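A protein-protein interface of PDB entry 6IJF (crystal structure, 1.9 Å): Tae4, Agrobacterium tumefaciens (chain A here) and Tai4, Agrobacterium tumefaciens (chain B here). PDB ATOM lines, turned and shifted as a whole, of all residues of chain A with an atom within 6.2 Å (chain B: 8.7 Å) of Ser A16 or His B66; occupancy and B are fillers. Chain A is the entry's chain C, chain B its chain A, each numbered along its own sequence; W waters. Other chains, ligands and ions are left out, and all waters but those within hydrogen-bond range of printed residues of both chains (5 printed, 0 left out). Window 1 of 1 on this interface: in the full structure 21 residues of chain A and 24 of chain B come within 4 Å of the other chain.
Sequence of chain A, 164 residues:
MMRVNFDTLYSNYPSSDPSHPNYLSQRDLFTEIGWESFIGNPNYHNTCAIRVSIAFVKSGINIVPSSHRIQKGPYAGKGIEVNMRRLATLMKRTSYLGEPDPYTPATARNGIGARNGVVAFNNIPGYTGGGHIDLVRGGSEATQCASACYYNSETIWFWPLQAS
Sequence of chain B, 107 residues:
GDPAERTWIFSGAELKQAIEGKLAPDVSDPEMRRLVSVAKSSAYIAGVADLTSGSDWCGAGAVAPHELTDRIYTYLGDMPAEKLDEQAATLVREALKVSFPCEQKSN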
ATOM      1  N   TYR A  13      18.201   0.979  -3.515  1.00  0.00           N
ATOM      2  CA  TYR A  13      16.796   0.755  -3.065  1.00  0.00           C
ATOM      3  C   TYR A  13      16.352   1.906  -2.160  1.00  0.00           C
ATOM      4  O   TYR A  13      16.963   2.156  -1.116  1.00  0.00           O
ATOM      5  CB  TYR A  13      16.649  -0.609  -2.382  1.00  0.00           C
ATOM      6  CG  TYR A  13      15.269  -0.837  -1.796  1.00  0.00           C
ATOM      7  CD1 TYR A  13      14.217  -1.294  -2.571  1.00  0.00           C
ATOM      8  CD2 TYR A  13      15.007  -0.547  -0.467  1.00  0.00           C
ATOM      9  CE1 TYR A  13      12.956  -1.474  -2.045  1.00  0.00           C
ATOM     10  CE2 TYR A  13      13.752  -0.763   0.089  1.00  0.00           C
ATOM     11  CZ  TYR A  13      12.715  -1.214  -0.706  1.00  0.00           C
ATOM     12  OH  TYR A  13      11.470  -1.338  -0.154  1.00  0.00           O
ATOM     13  N   PRO A  14      15.256   2.617  -2.500  1.00  0.00           N
ATOM     14  CA  PRO A  14      14.650   3.596  -1.591  1.00  0.00           C
ATOM     15  C   PRO A  14      13.648   2.955  -0.616  1.00  0.00           C
ATOM     16  O   PRO A  14      12.623   2.386  -1.031  1.00  0.00           O
ATOM     17  CB  PRO A  14      13.994   4.562  -2.591  1.00  0.00           C
ATOM     18  CG  PRO A  14      13.499   3.656  -3.680  1.00  0.00           C
ATOM     19  CD  PRO A  14      14.508   2.516  -3.760  1.00  0.00           C
ATOM     20  N   SER A  15      13.938   3.019   0.678  1.00  0.00           N
ATOM     21  CA  SER A  15      13.137   2.346   1.731  1.00  0.00           C
ATOM     22  C   SER A  15      11.960   3.224   2.161  1.00  0.00           C
ATOM     23  O   SER A  15      12.103   4.464   2.205  1.00  0.00           O
ATOM     24  CB  SER A  15      14.042   1.972   2.886  1.00  0.00           C
ATOM     25  OG  SER A  15      13.288   1.586   4.030  1.00  0.00           O
ATOM     26  N   SER A  16      10.825   2.629   2.537  1.00  0.00           N
ATOM     27  CA  SER A  16       9.678   3.352   3.154  1.00  0.00           C
ATOM     28  C   SER A  16       9.812   3.414   4.692  1.00  0.00           C
ATOM     29  O   SER A  16       8.892   3.957   5.352  1.00  0.00           O
ATOM     30  CB  SER A  16       8.350   2.723   2.754  1.00  0.00           C
ATOM     31  OG  SER A  16       8.346   1.355   3.060  1.00  0.00           O
ATOM     32  N   ASP A  17      10.903   2.882   5.252  1.00  0.00           N
ATOM     33  CA  ASP A  17      11.129   2.777   6.715  1.00  0.00           C
ATOM     34  C   ASP A  17      11.994   3.953   7.153  1.00  0.00           C
ATOM     35  O   ASP A  17      13.169   4.024   6.809  1.00  0.00           O
ATOM     36  CB  ASP A  17      11.741   1.428   7.078  1.00  0.00           C
ATOM     37  CG  ASP A  17      12.054   1.251   8.565  1.00  0.00           C
ATOM     38  OD1 ASP A  17      11.843   2.172   9.347  1.00  0.00           O
ATOM     39  OD2 ASP A  17      12.495   0.181   8.924  1.00  0.00           O
ATOM     40  N   PRO A  18      11.432   4.926   7.898  1.00  0.00           N
ATOM     41  CA  PRO A  18      12.212   6.063   8.389  1.00  0.00           C
ATOM     42  C   PRO A  18      13.450   5.702   9.218  1.00  0.00           C
ATOM     43  O   PRO A  18      14.306   6.546   9.378  1.00  0.00           O
ATOM     44  CB  PRO A  18      11.188   6.808   9.259  1.00  0.00           C
ATOM     45  CG  PRO A  18       9.864   6.482   8.610  1.00  0.00           C
ATOM     46  CD  PRO A  18      10.006   5.024   8.240  1.00  0.00           C
ATOM     47  N   ASN A  22      18.408   4.430   3.816  1.00  0.00           N
ATOM     48  CA  ASN A  22      17.933   4.789   2.452  1.00  0.00           C
ATOM     49  C   ASN A  22      16.460   5.212   2.487  1.00  0.00           C
ATOM     50  O   ASN A  22      15.830   5.118   1.407  1.00  0.00           O
ATOM     51  CB  ASN A  22      18.007   3.623   1.459  1.00  0.00           C
ATOM     52  CG  ASN A  22      19.399   3.108   1.173  1.00  0.00           C
ATOM     53  OD1 ASN A  22      20.366   3.850   1.304  1.00  0.00           O
ATOM     54  ND2 ASN A  22      19.495   1.851   0.746  1.00  0.00           N
ATOM     55  N   TYR A  23      15.913   5.636   3.638  1.00  0.00           N
ATOM     56  CA  TYR A  23      14.513   6.145   3.708  1.00  0.00           C
ATOM     57  C   TYR A  23      14.285   7.252   2.671  1.00  0.00           C
ATOM     58  O   TYR A  23      15.044   8.221   2.585  1.00  0.00           O
ATOM     59  CB  TYR A  23      14.134   6.694   5.081  1.00  0.00           C
ATOM     60  CG  TYR A  23      12.760   7.333   5.175  1.00  0.00           C
ATOM     61  CD1 TYR A  23      11.597   6.607   4.922  1.00  0.00           C
ATOM     62  CD2 TYR A  23      12.607   8.660   5.568  1.00  0.00           C
ATOM     63  CE1 TYR A  23      10.335   7.188   5.027  1.00  0.00           C
ATOM     64  CE2 TYR A  23      11.353   9.254   5.689  1.00  0.00           C
ATOM     65  CZ  TYR A  23      10.208   8.514   5.430  1.00  0.00           C
ATOM     66  OH  TYR A  23       8.955   9.073   5.553  1.00  0.00           O
ATOM     67  N   LEU A  24      13.142   7.176   2.002  1.00  0.00           N
ATOM     68  CA  LEU A  24      12.600   8.202   1.101  1.00  0.00           C
ATOM     69  C   LEU A  24      11.073   8.108   1.192  1.00  0.00           C
ATOM     70  O   LEU A  24      10.559   6.992   0.948  1.00  0.00           O
ATOM     71  CB  LEU A  24      13.166   7.875  -0.290  1.00  0.00           C
ATOM     72  CG  LEU A  24      13.191   9.019  -1.299  1.00  0.00           C
ATOM     73  CD1 LEU A  24      14.151  10.106  -0.824  1.00  0.00           C
ATOM     74  CD2 LEU A  24      13.558   8.495  -2.690  1.00  0.00           C
ATOM     75  N   SER A  25      10.406   9.157   1.688  1.00  0.00           N
ATOM     76  CA  SER A  25       8.934   9.229   1.874  1.00  0.00           C
ATOM     77  C   SER A  25       8.239   9.011   0.532  1.00  0.00           C
ATOM     78  O   SER A  25       8.903   9.193  -0.532  1.00  0.00           O
ATOM     79  CB  SER A  25       8.511  10.563   2.460  1.00  0.00           C
ATOM     80  OG  SER A  25       8.752  11.574   1.512  1.00  0.00           O
ATOM     81  N   ASN A  46       0.378   2.052  -2.100  1.00  0.00           N
ATOM     82  CA  ASN A  46       1.262   0.885  -1.856  1.00  0.00           C
ATOM     83  C   ASN A  46       2.464   0.998  -2.798  1.00  0.00           C
ATOM     84  O   ASN A  46       2.296   0.826  -4.006  1.00  0.00           O
ATOM     85  CB  ASN A  46       0.486  -0.430  -1.926  1.00  0.00           C
ATOM     86  CG  ASN A  46      -0.652  -0.439  -0.930  1.00  0.00           C
ATOM     87  OD1 ASN A  46      -1.790  -0.717  -1.301  1.00  0.00           O
ATOM     88  ND2 ASN A  46      -0.371  -0.050   0.299  1.00  0.00           N
ATOM     89  N   THR A  47       3.635   1.321  -2.260  1.00  0.00           N
ATOM     90  CA  THR A  47       4.834   1.733  -3.046  1.00  0.00           C
ATOM     91  C   THR A  47       5.840   0.598  -3.188  1.00  0.00           C
ATOM     92  O   THR A  47       6.873   0.834  -3.845  1.00  0.00           O
ATOM     93  CB  THR A  47       5.455   2.975  -2.384  1.00  0.00           C
ATOM     94  OG1 THR A  47       5.896   2.572  -1.086  1.00  0.00           O
ATOM     95  CG2 THR A  47       4.481   4.131  -2.273  1.00  0.00           C
ATOM     96  N   CYS A  48       5.587  -0.603  -2.637  1.00  0.00           N
ATOM     97  CA  CYS A  48       6.661  -1.636  -2.484  1.00  0.00           C
ATOM     98  C   CYS A  48       7.228  -2.017  -3.854  1.00  0.00           C
ATOM     99  O   CYS A  48       8.472  -2.116  -3.964  1.00  0.00           O
ATOM    100  CB  CYS A  48       6.194  -2.867  -1.715  1.00  0.00           C
ATOM    101  SG  CYS A  48       4.923  -3.886  -2.539  1.00  0.00           S
ATOM    102  N   ARG A  51       9.384   0.745  -5.460  1.00  0.00           N
ATOM    103  CA  ARG A  51      10.701   0.854  -4.781  1.00  0.00           C
ATOM    104  C   ARG A  51      11.614  -0.257  -5.303  1.00  0.00           C
ATOM    105  O   ARG A  51      12.793   0.019  -5.625  1.00  0.00           O
ATOM    106  CB  ARG A  51      10.508   0.844  -3.258  1.00  0.00           C
ATOM    107  CG  ARG A  51       9.744   2.055  -2.761  1.00  0.00           C
ATOM    108  CD  ARG A  51       9.390   1.987  -1.282  1.00  0.00           C
ATOM    109  NE  ARG A  51       8.664   3.167  -0.850  1.00  0.00           N
ATOM    110  CZ  ARG A  51       9.237   4.305  -0.465  1.00  0.00           C
ATOM    111  NH1 ARG A  51      10.556   4.418  -0.485  1.00  0.00           N
ATOM    112  NH2 ARG A  51       8.491   5.300  -0.027  1.00  0.00           N
ATOM    113  N   HIS A 132       3.590  -8.066  -0.399  1.00  0.00           N
ATOM    114  CA  HIS A 132       4.722  -7.126  -0.204  1.00  0.00           C
ATOM    115  C   HIS A 132       5.947  -7.736  -0.858  1.00  0.00           C
ATOM    116  O   HIS A 132       6.217  -8.929  -0.648  1.00  0.00           O
ATOM    117  CB  HIS A 132       4.944  -6.855   1.286  1.00  0.00           C
ATOM    118  CG  HIS A 132       6.062  -5.908   1.564  1.00  0.00           C
ATOM    119  ND1 HIS A 132       5.977  -4.581   1.227  1.00  0.00           N
ATOM    120  CD2 HIS A 132       7.283  -6.102   2.116  1.00  0.00           C
ATOM    121  CE1 HIS A 132       7.111  -3.979   1.562  1.00  0.00           C
ATOM    122  NE2 HIS A 132       7.921  -4.885   2.137  1.00  0.00           N
ATOM    123  N   ALA A 146      14.372  -4.361   3.948  1.00  0.00           N
ATOM    124  CA  ALA A 146      14.737  -2.950   3.724  1.00  0.00           C
ATOM    125  C   ALA A 146      13.576  -2.026   4.100  1.00  0.00           C
ATOM    126  O   ALA A 146      13.858  -0.943   4.669  1.00  0.00           O
ATOM    127  CB  ALA A 146      15.190  -2.769   2.295  1.00  0.00           C
ATOM    128  N   SER A 147      12.330  -2.408   3.801  1.00  0.00           N
ATOM    129  CA  SER A 147      11.124  -1.607   4.118  1.00  0.00           C
ATOM    130  C   SER A 147      10.245  -2.258   5.192  1.00  0.00           C
ATOM    131  O   SER A 147       9.852  -1.549   6.143  1.00  0.00           O
ATOM    132  CB  SER A 147      10.333  -1.319   2.890  1.00  0.00           C
ATOM    133  OG  SER A 147      10.926  -0.298   2.154  1.00  0.00           O
ATOM    134  N   ALA A 148       9.914  -3.541   5.078  1.00  0.00           N
ATOM    135  CA  ALA A 148       9.025  -4.220   6.046  1.00  0.00           C
ATOM    136  C   ALA A 148       9.001  -5.714   5.762  1.00  0.00           C
ATOM    137  O   ALA A 148       9.103  -6.082   4.597  1.00  0.00           O
ATOM    138  CB  ALA A 148       7.631  -3.636   5.901  1.00  0.00           C
ATOM    139  N   TYR A 150       6.566  -9.310   6.367  1.00  0.00           N
ATOM    140  CA  TYR A 150       5.160  -9.714   6.643  1.00  0.00           C
ATOM    141  C   TYR A 150       5.102 -11.238   6.763  1.00  0.00           C
ATOM    142  O   TYR A 150       4.620 -11.929   5.868  1.00  0.00           O
ATOM    143  CB  TYR A 150       4.217  -9.217   5.551  1.00  0.00           C
ATOM    144  CG  TYR A 150       3.941  -7.748   5.648  1.00  0.00           C
ATOM    145  CD1 TYR A 150       2.967  -7.264   6.506  1.00  0.00           C
ATOM    146  CD2 TYR A 150       4.667  -6.840   4.897  1.00  0.00           C
ATOM    147  CE1 TYR A 150       2.688  -5.913   6.586  1.00  0.00           C
ATOM    148  CE2 TYR A 150       4.407  -5.485   4.984  1.00  0.00           C
ATOM    149  CZ  TYR A 150       3.404  -5.021   5.812  1.00  0.00           C
ATOM    150  OH  TYR A 150       3.198  -3.684   5.919  1.00  0.00           O
ATOM    151  N   ILE B  19       9.796   5.234  15.619  1.00  0.00           N
ATOM    152  CA  ILE B  19       9.702   5.123  14.137  1.00  0.00           C
ATOM    153  C   ILE B  19      11.118   5.200  13.535  1.00  0.00           C
ATOM    154  O   ILE B  19      11.399   4.483  12.568  1.00  0.00           O
ATOM    155  CB  ILE B  19       8.750   6.188  13.557  1.00  0.00           C
ATOM    156  CG1 ILE B  19       7.301   5.945  13.978  1.00  0.00           C
ATOM    157  CG2 ILE B  19       8.889   6.240  12.030  1.00  0.00           C
ATOM    158  CD1 ILE B  19       6.329   7.077  13.674  1.00  0.00           C
ATOM    159  N   VAL B  38      11.026  -0.135  15.968  1.00  0.00           N
ATOM    160  CA  VAL B  38      10.092  -0.059  14.824  1.00  0.00           C
ATOM    161  C   VAL B  38       8.878  -0.960  15.107  1.00  0.00           C
ATOM    162  O   VAL B  38       7.755  -0.559  14.711  1.00  0.00           O
ATOM    163  CB  VAL B  38      10.823  -0.378  13.509  1.00  0.00           C
ATOM    164  CG1 VAL B  38       9.852  -0.492  12.342  1.00  0.00           C
ATOM    165  CG2 VAL B  38      11.892   0.663  13.194  1.00  0.00           C
ATOM    166  N   SER B  42       5.127   0.599  14.952  1.00  0.00           N
ATOM    167  CA  SER B  42       4.173  -0.059  14.027  1.00  0.00           C
ATOM    168  C   SER B  42       2.930  -0.502  14.794  1.00  0.00           C
ATOM    169  O   SER B  42       1.826  -0.281  14.300  1.00  0.00           O
ATOM    170  CB  SER B  42       4.790  -1.218  13.317  1.00  0.00           C
ATOM    171  OG  SER B  42       5.913  -0.760  12.593  1.00  0.00           O
ATOM    172  N   ILE B  45       0.770   2.457  16.239  1.00  0.00           N
ATOM    173  CA  ILE B  45       0.030   2.978  15.056  1.00  0.00           C
ATOM    174  C   ILE B  45      -1.110   2.016  14.690  1.00  0.00           C
ATOM    175  O   ILE B  45      -2.231   2.494  14.446  1.00  0.00           O
ATOM    176  CB  ILE B  45       0.991   3.220  13.882  1.00  0.00           C
ATOM    177  CG1 ILE B  45       1.885   4.419  14.189  1.00  0.00           C
ATOM    178  CG2 ILE B  45       0.201   3.353  12.581  1.00  0.00           C
ATOM    179  CD1 ILE B  45       3.064   4.569  13.285  1.00  0.00           C
ATOM    180  N   ALA B  46      -0.858   0.711  14.680  1.00  0.00           N
ATOM    181  CA  ALA B  46      -1.886  -0.296  14.352  1.00  0.00           C
ATOM    182  C   ALA B  46      -3.065  -0.210  15.340  1.00  0.00           C
ATOM    183  O   ALA B  46      -4.205  -0.468  14.906  1.00  0.00           O
ATOM    184  CB  ALA B  46      -1.296  -1.688  14.353  1.00  0.00           C
ATOM    185  N   VAL B  63      -4.612  -0.672   2.247  1.00  0.00           N
ATOM    186  CA  VAL B  63      -3.295  -0.002   2.460  1.00  0.00           C
ATOM    187  C   VAL B  63      -2.406  -0.871   3.353  1.00  0.00           C
ATOM    188  O   VAL B  63      -2.808  -1.195   4.468  1.00  0.00           O
ATOM    189  CB  VAL B  63      -3.458   1.412   3.024  1.00  0.00           C
ATOM    190  CG1 VAL B  63      -2.092   2.038   3.301  1.00  0.00           C
ATOM    191  CG2 VAL B  63      -4.279   2.275   2.082  1.00  0.00           C
ATOM    192  N   ALA B  64      -1.225  -1.225   2.863  1.00  0.00           N
ATOM    193  CA  ALA B  64      -0.227  -2.004   3.629  1.00  0.00           C
ATOM    194  C   ALA B  64       0.056  -1.266   4.923  1.00  0.00           C
ATOM    195  O   ALA B  64       0.220  -0.040   4.929  1.00  0.00           O
ATOM    196  CB  ALA B  64       1.028  -2.223   2.827  1.00  0.00           C
ATOM    197  N   PRO B  65       0.117  -1.968   6.076  1.00  0.00           N
ATOM    198  CA  PRO B  65       0.381  -1.300   7.351  1.00  0.00           C
ATOM    199  C   PRO B  65       1.606  -0.362   7.416  1.00  0.00           C
ATOM    200  O   PRO B  65       1.527   0.715   7.989  1.00  0.00           O
ATOM    201  CB  PRO B  65       0.544  -2.470   8.345  1.00  0.00           C
ATOM    202  CG  PRO B  65      -0.230  -3.624   7.706  1.00  0.00           C
ATOM    203  CD  PRO B  65      -0.125  -3.414   6.207  1.00  0.00           C
ATOM    204  N   HIS B  66       2.722  -0.743   6.802  1.00  0.00           N
ATOM    205  CA  HIS B  66       3.975   0.063   6.853  1.00  0.00           C
ATOM    206  C   HIS B  66       3.788   1.371   6.071  1.00  0.00           C
ATOM    207  O   HIS B  66       4.531   2.335   6.330  1.00  0.00           O
ATOM    208  CB  HIS B  66       5.160  -0.772   6.345  1.00  0.00           C
ATOM    209  CG  HIS B  66       5.122  -1.008   4.870  1.00  0.00           C
ATOM    210  ND1 HIS B  66       4.445  -2.081   4.322  1.00  0.00           N
ATOM    211  CD2 HIS B  66       5.670  -0.319   3.839  1.00  0.00           C
ATOM    212  CE1 HIS B  66       4.573  -2.052   3.007  1.00  0.00           C
ATOM    213  NE2 HIS B  66       5.330  -0.963   2.674  1.00  0.00           N
ATOM    214  N   GLU B  67       2.840   1.436   5.137  1.00  0.00           N
ATOM    215  CA  GLU B  67       2.553   2.693   4.419  1.00  0.00           C
ATOM    216  C   GLU B  67       1.945   3.685   5.399  1.00  0.00           C
ATOM    217  O   GLU B  67       2.185   4.898   5.234  1.00  0.00           O
ATOM    218  CB  GLU B  67       1.645   2.474   3.200  1.00  0.00           C
ATOM    219  CG  GLU B  67       2.317   1.644   2.130  1.00  0.00           C
ATOM    220  CD  GLU B  67       3.446   2.302   1.346  1.00  0.00           C
ATOM    221  OE1 GLU B  67       3.702   3.490   1.574  1.00  0.00           O
ATOM    222  OE2 GLU B  67       4.023   1.643   0.461  1.00  0.00           O
ATOM    223  N   LEU B  68       1.169   3.218   6.372  1.00  0.00           N
ATOM    224  CA  LEU B  68       0.619   4.155   7.381  1.00  0.00           C
ATOM    225  C   LEU B  68       1.785   4.835   8.107  1.00  0.00           C
ATOM    226  O   LEU B  68       1.720   6.060   8.359  1.00  0.00           O
ATOM    227  CB  LEU B  68      -0.273   3.411   8.373  1.00  0.00           C
ATOM    228  CG  LEU B  68      -1.421   2.603   7.774  1.00  0.00           C
ATOM    229  CD1 LEU B  68      -2.209   1.948   8.892  1.00  0.00           C
ATOM    230  CD2 LEU B  68      -2.333   3.474   6.926  1.00  0.00           C
ATOM    231  N   THR B  69       2.812   4.063   8.468  1.00  0.00           N
ATOM    232  CA  THR B  69       3.955   4.593   9.251  1.00  0.00           C
ATOM    233  C   THR B  69       4.650   5.702   8.464  1.00  0.00           C
ATOM    234  O   THR B  69       4.988   6.751   9.066  1.00  0.00           O
ATOM    235  CB  THR B  69       4.895   3.460   9.665  1.00  0.00           C
ATOM    236  OG1 THR B  69       4.107   2.593  10.482  1.00  0.00           O
ATOM    237  CG2 THR B  69       6.103   3.965  10.420  1.00  0.00           C
ATOM    238  N   ASP B  70       4.829   5.510   7.154  1.00  0.00           N
ATOM    239  CA  ASP B  70       5.471   6.509   6.273  1.00  0.00           C
ATOM    240  C   ASP B  70       4.663   7.816   6.350  1.00  0.00           C
ATOM    241  O   ASP B  70       5.262   8.851   6.566  1.00  0.00           O
ATOM    242  CB  ASP B  70       5.603   6.003   4.833  1.00  0.00           C
ATOM    243  CG  ASP B  70       6.060   7.086   3.857  1.00  0.00           C
ATOM    244  OD1 ASP B  70       7.035   7.807   4.198  1.00  0.00           O
ATOM    245  OD2 ASP B  70       5.422   7.234   2.783  1.00  0.00           O
ATOM    246  N   ARG B  71       3.340   7.768   6.216  1.00  0.00           N
ATOM    247  CA  ARG B  71       2.514   9.011   6.190  1.00  0.00           C
ATOM    248  C   ARG B  71       2.494   9.644   7.578  1.00  0.00           C
ATOM    249  O   ARG B  71       2.556  10.878   7.674  1.00  0.00           O
ATOM    250  CB  ARG B  71       1.070   8.758   5.733  1.00  0.00           C
ATOM    251  CG  ARG B  71       0.940   7.984   4.427  1.00  0.00           C
ATOM    252  CD  ARG B  71       1.630   8.569   3.186  1.00  0.00           C
ATOM    253  NE  ARG B  71       1.174   7.762   2.064  1.00  0.00           N
ATOM    254  CZ  ARG B  71       1.667   6.596   1.665  1.00  0.00           C
ATOM    255  NH1 ARG B  71       1.045   5.943   0.698  1.00  0.00           N
ATOM    256  NH2 ARG B  71       2.794   6.105   2.176  1.00  0.00           N
ATOM    257  N   ILE B  72       2.448   8.833   8.632  1.00  0.00           N
ATOM    258  CA  ILE B  72       2.440   9.376  10.019  1.00  0.00           C
ATOM    259  C   ILE B  72       3.766  10.094  10.275  1.00  0.00           C
ATOM    260  O   ILE B  72       3.762  11.178  10.849  1.00  0.00           O
ATOM    261  CB  ILE B  72       2.135   8.242  11.011  1.00  0.00           C
ATOM    262  CG1 ILE B  72       0.641   7.923  10.959  1.00  0.00           C
ATOM    263  CG2 ILE B  72       2.631   8.564  12.412  1.00  0.00           C
ATOM    264  CD1 ILE B  72       0.302   6.593  11.487  1.00  0.00           C
ATOM    265  N   TYR B  73       4.878   9.503   9.871  1.00  0.00           N
ATOM    266  CA  TYR B  73       6.216  10.088  10.096  1.00  0.00           C
ATOM    267  C   TYR B  73       6.316  11.453   9.409  1.00  0.00           C
ATOM    268  O   TYR B  73       6.799  12.418  10.035  1.00  0.00           O
ATOM    269  CB  TYR B  73       7.316   9.173   9.584  1.00  0.00           C
ATOM    270  CG  TYR B  73       8.690   9.695   9.896  1.00  0.00           C
ATOM    271  CD1 TYR B  73       9.127   9.749  11.202  1.00  0.00           C
ATOM    272  CD2 TYR B  73       9.540  10.150   8.898  1.00  0.00           C
ATOM    273  CE1 TYR B  73      10.405  10.190  11.521  1.00  0.00           C
ATOM    274  CE2 TYR B  73      10.832  10.579   9.195  1.00  0.00           C
ATOM    275  CZ  TYR B  73      11.259  10.589  10.509  1.00  0.00           C
ATOM    276  OH  TYR B  73      12.507  11.014  10.849  1.00  0.00           O
ATOM    277  N   THR B  74       5.876  11.570   8.165  1.00  0.00           N
ATOM    278  CA  THR B  74       5.973  12.870   7.448  1.00  0.00           C
ATOM    279  C   THR B  74       5.092  13.887   8.184  1.00  0.00           C
ATOM    280  O   THR B  74       5.536  15.017   8.346  1.00  0.00           O
ATOM    281  CB  THR B  74       5.599  12.701   5.966  1.00  0.00           C
ATOM    282  OG1 THR B  74       4.200  12.448   5.966  1.00  0.00           O
ATOM    283  CG2 THR B  74       6.335  11.581   5.268  1.00  0.00           C
ATOM    284  N   PHE B 100      -5.467   9.727   4.607  1.00  0.00           N
ATOM    285  CA  PHE B 100      -6.442   8.697   4.144  1.00  0.00           C
ATOM    286  C   PHE B 100      -7.860   9.181   4.454  1.00  0.00           C
ATOM    287  O   PHE B 100      -8.638   8.512   5.143  1.00  0.00           O
ATOM    288  CB  PHE B 100      -6.128   7.340   4.782  1.00  0.00           C
ATOM    289  CG  PHE B 100      -4.714   6.855   4.573  1.00  0.00           C
ATOM    290  CD1 PHE B 100      -4.355   6.218   3.401  1.00  0.00           C
ATOM    291  CD2 PHE B 100      -3.743   7.033   5.551  1.00  0.00           C
ATOM    292  CE1 PHE B 100      -3.052   5.786   3.203  1.00  0.00           C
ATOM    293  CE2 PHE B 100      -2.431   6.612   5.347  1.00  0.00           C
ATOM    294  CZ  PHE B 100      -2.094   5.977   4.173  1.00  0.00           C
HETATM  295  O   HOH W   1       5.802   5.066   1.055  1.00  0.00           O
HETATM  296  O   HOH W   2       3.585  -1.168  -0.327  1.00  0.00           O
HETATM  297  O   HOH W   3       9.791   2.797  11.161  1.00  0.00           O
HETATM  298  O   HOH W   4       7.182  -0.171   0.631  1.00  0.00           O
HETATM  299  O   HOH W   5       7.126   2.552   7.030  1.00  0.00           O
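Of chain B, only His B66 and Asp B70 come within 4 Å of Ser A16.
Of chain A, only Ser A16 (3.3 Å), His A132 (3.4 Å), Ala A148 (3.8 Å) and Tyr A150 (2.6 Å) come within 4 Å of His B66.
No residue of chain B comes within 4 Å of Ser A15.
Of the printed residues of chain B, Tyr A150 touches Pro B65 (3.3 Å) and His B66 (2.6 Å).
Printed residues of chain A within 4 Å of Ile B19: Asp A17 (3.99 Å) and Pro A18 (3.6 Å).
Of the printed residues of chain A, Asp B70 touches Ser A16, Tyr A23 and Ser A25.
Printed residues of chain A within 4 Å of Tyr B73: Pro A18 and Tyr A23.
Of the printed residues of chain B, Pro A18 touches Ile B19 (3.6 Å) and Tyr B73 (3.7 Å).
The nearest printed residue of chain A that does not touch Thr B74 is Pro A18 (6.5 Å).
OG1 of Thr A47 lies within hydrogen-bond range of NE of Arg A51 (2.8 Å).
NH2 of Arg B71 is in salt-bridge range of OE1 of Glu B67 (2.8 Å).
A ring nitrogen (NE2) of His A132 lies within hydrogen-bond range of the backbone carbonyl oxygen (O) of Ala A148 (3.0 Å).
OD2 of Asp B70 lies within salt-bridge range of NH2 of Arg B71 (2.9 Å).
The side-chain hydroxyl (OG) of Ser A15 lies within hydrogen-bond range of the backbone NH (N) of Asp A17.
The side-chain hydroxyl (OG) of Ser A147 lies within hydrogen-bond range of the backbone NH (N) of Ser A16 (3.0 Å).
The backbone NH (N) of Ala B64 sits close to the side-chain amide nitrogen (ND2) of Asn A46.
A ring nitrogen (ND1) of His B66 lies within hydrogen-bond range of the side-chain hydroxyl (OH) of Tyr A150.
The side-chain hydroxyl of Tyr A23 sits at hydrogen-bond distance from the side-chain carboxylate of Asp B70.
The side-chain hydroxyl (OG1) of Thr A47 is in hydrogen-bond range of the side-chain carboxylate (OE2) of Glu B67, at 2.6 Å.
Among the printed residues, merely in contact across the chains: Ser A16 with His B66, Ser A16 with Asp B70, Asp A17 with Ile B19, Pro A18 with Ile B19, Pro A18 with Tyr B73, Tyr A23 with Tyr B73, Tyr A23 with Thr B74, Ser A25 with Asp B70, Ser A25 with Thr B74, Asn A46 with Val B63, Asn A46 with Glu B67, His A132 with His B66, Ala A148 with His B66 and Tyr A150 with Pro B65.
Water W1 lies within hydrogen-bond range of OE1 of Glu B67, OD2 of Asp B70, NH2 of Arg A51, OG1 of Thr A47 and NH2 of Arg B71.
Water W5 lies within hydrogen-bond range of the backbone carbonyl oxygen (O) of His B66 (2.7 Å) and the backbone carbonyl oxygen (O) of Ser A16 (2.8 Å).
Water W3 lies within hydrogen-bond range of the backbone carbonyl oxygen (O) of Ile B19 (2.7 Å) and the side-chain carboxylate (OD1) of Asp A17 (2.8 Å).
Water W4 lies within hydrogen-bond range of a ring nitrogen (NE2) of His B66 (2.9 Å), the side-chain hydroxyl (OG) of Ser A16 (3.1 Å) and the side-chain hydroxyl (OG1) of Thr A47 (3.5 Å).
Water W2 lies within hydrogen-bond range of the side-chain carboxylate (OE2) of Glu B67 (3.0 Å), the backbone NH (N) of Cys A48 (3.1 Å), the backbone NH (N) of Thr A47 (3.2 Å) and a ring nitrogen (NE2) of His B66 (3.5 Å).
Hydrophobic or aromatic side chains of chain A that line the printed part of chain B: Pro A18, Tyr A23, His A132, Ala A148 and Tyr A150.
Among the printed residues, 18 pairs touch across the chains.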
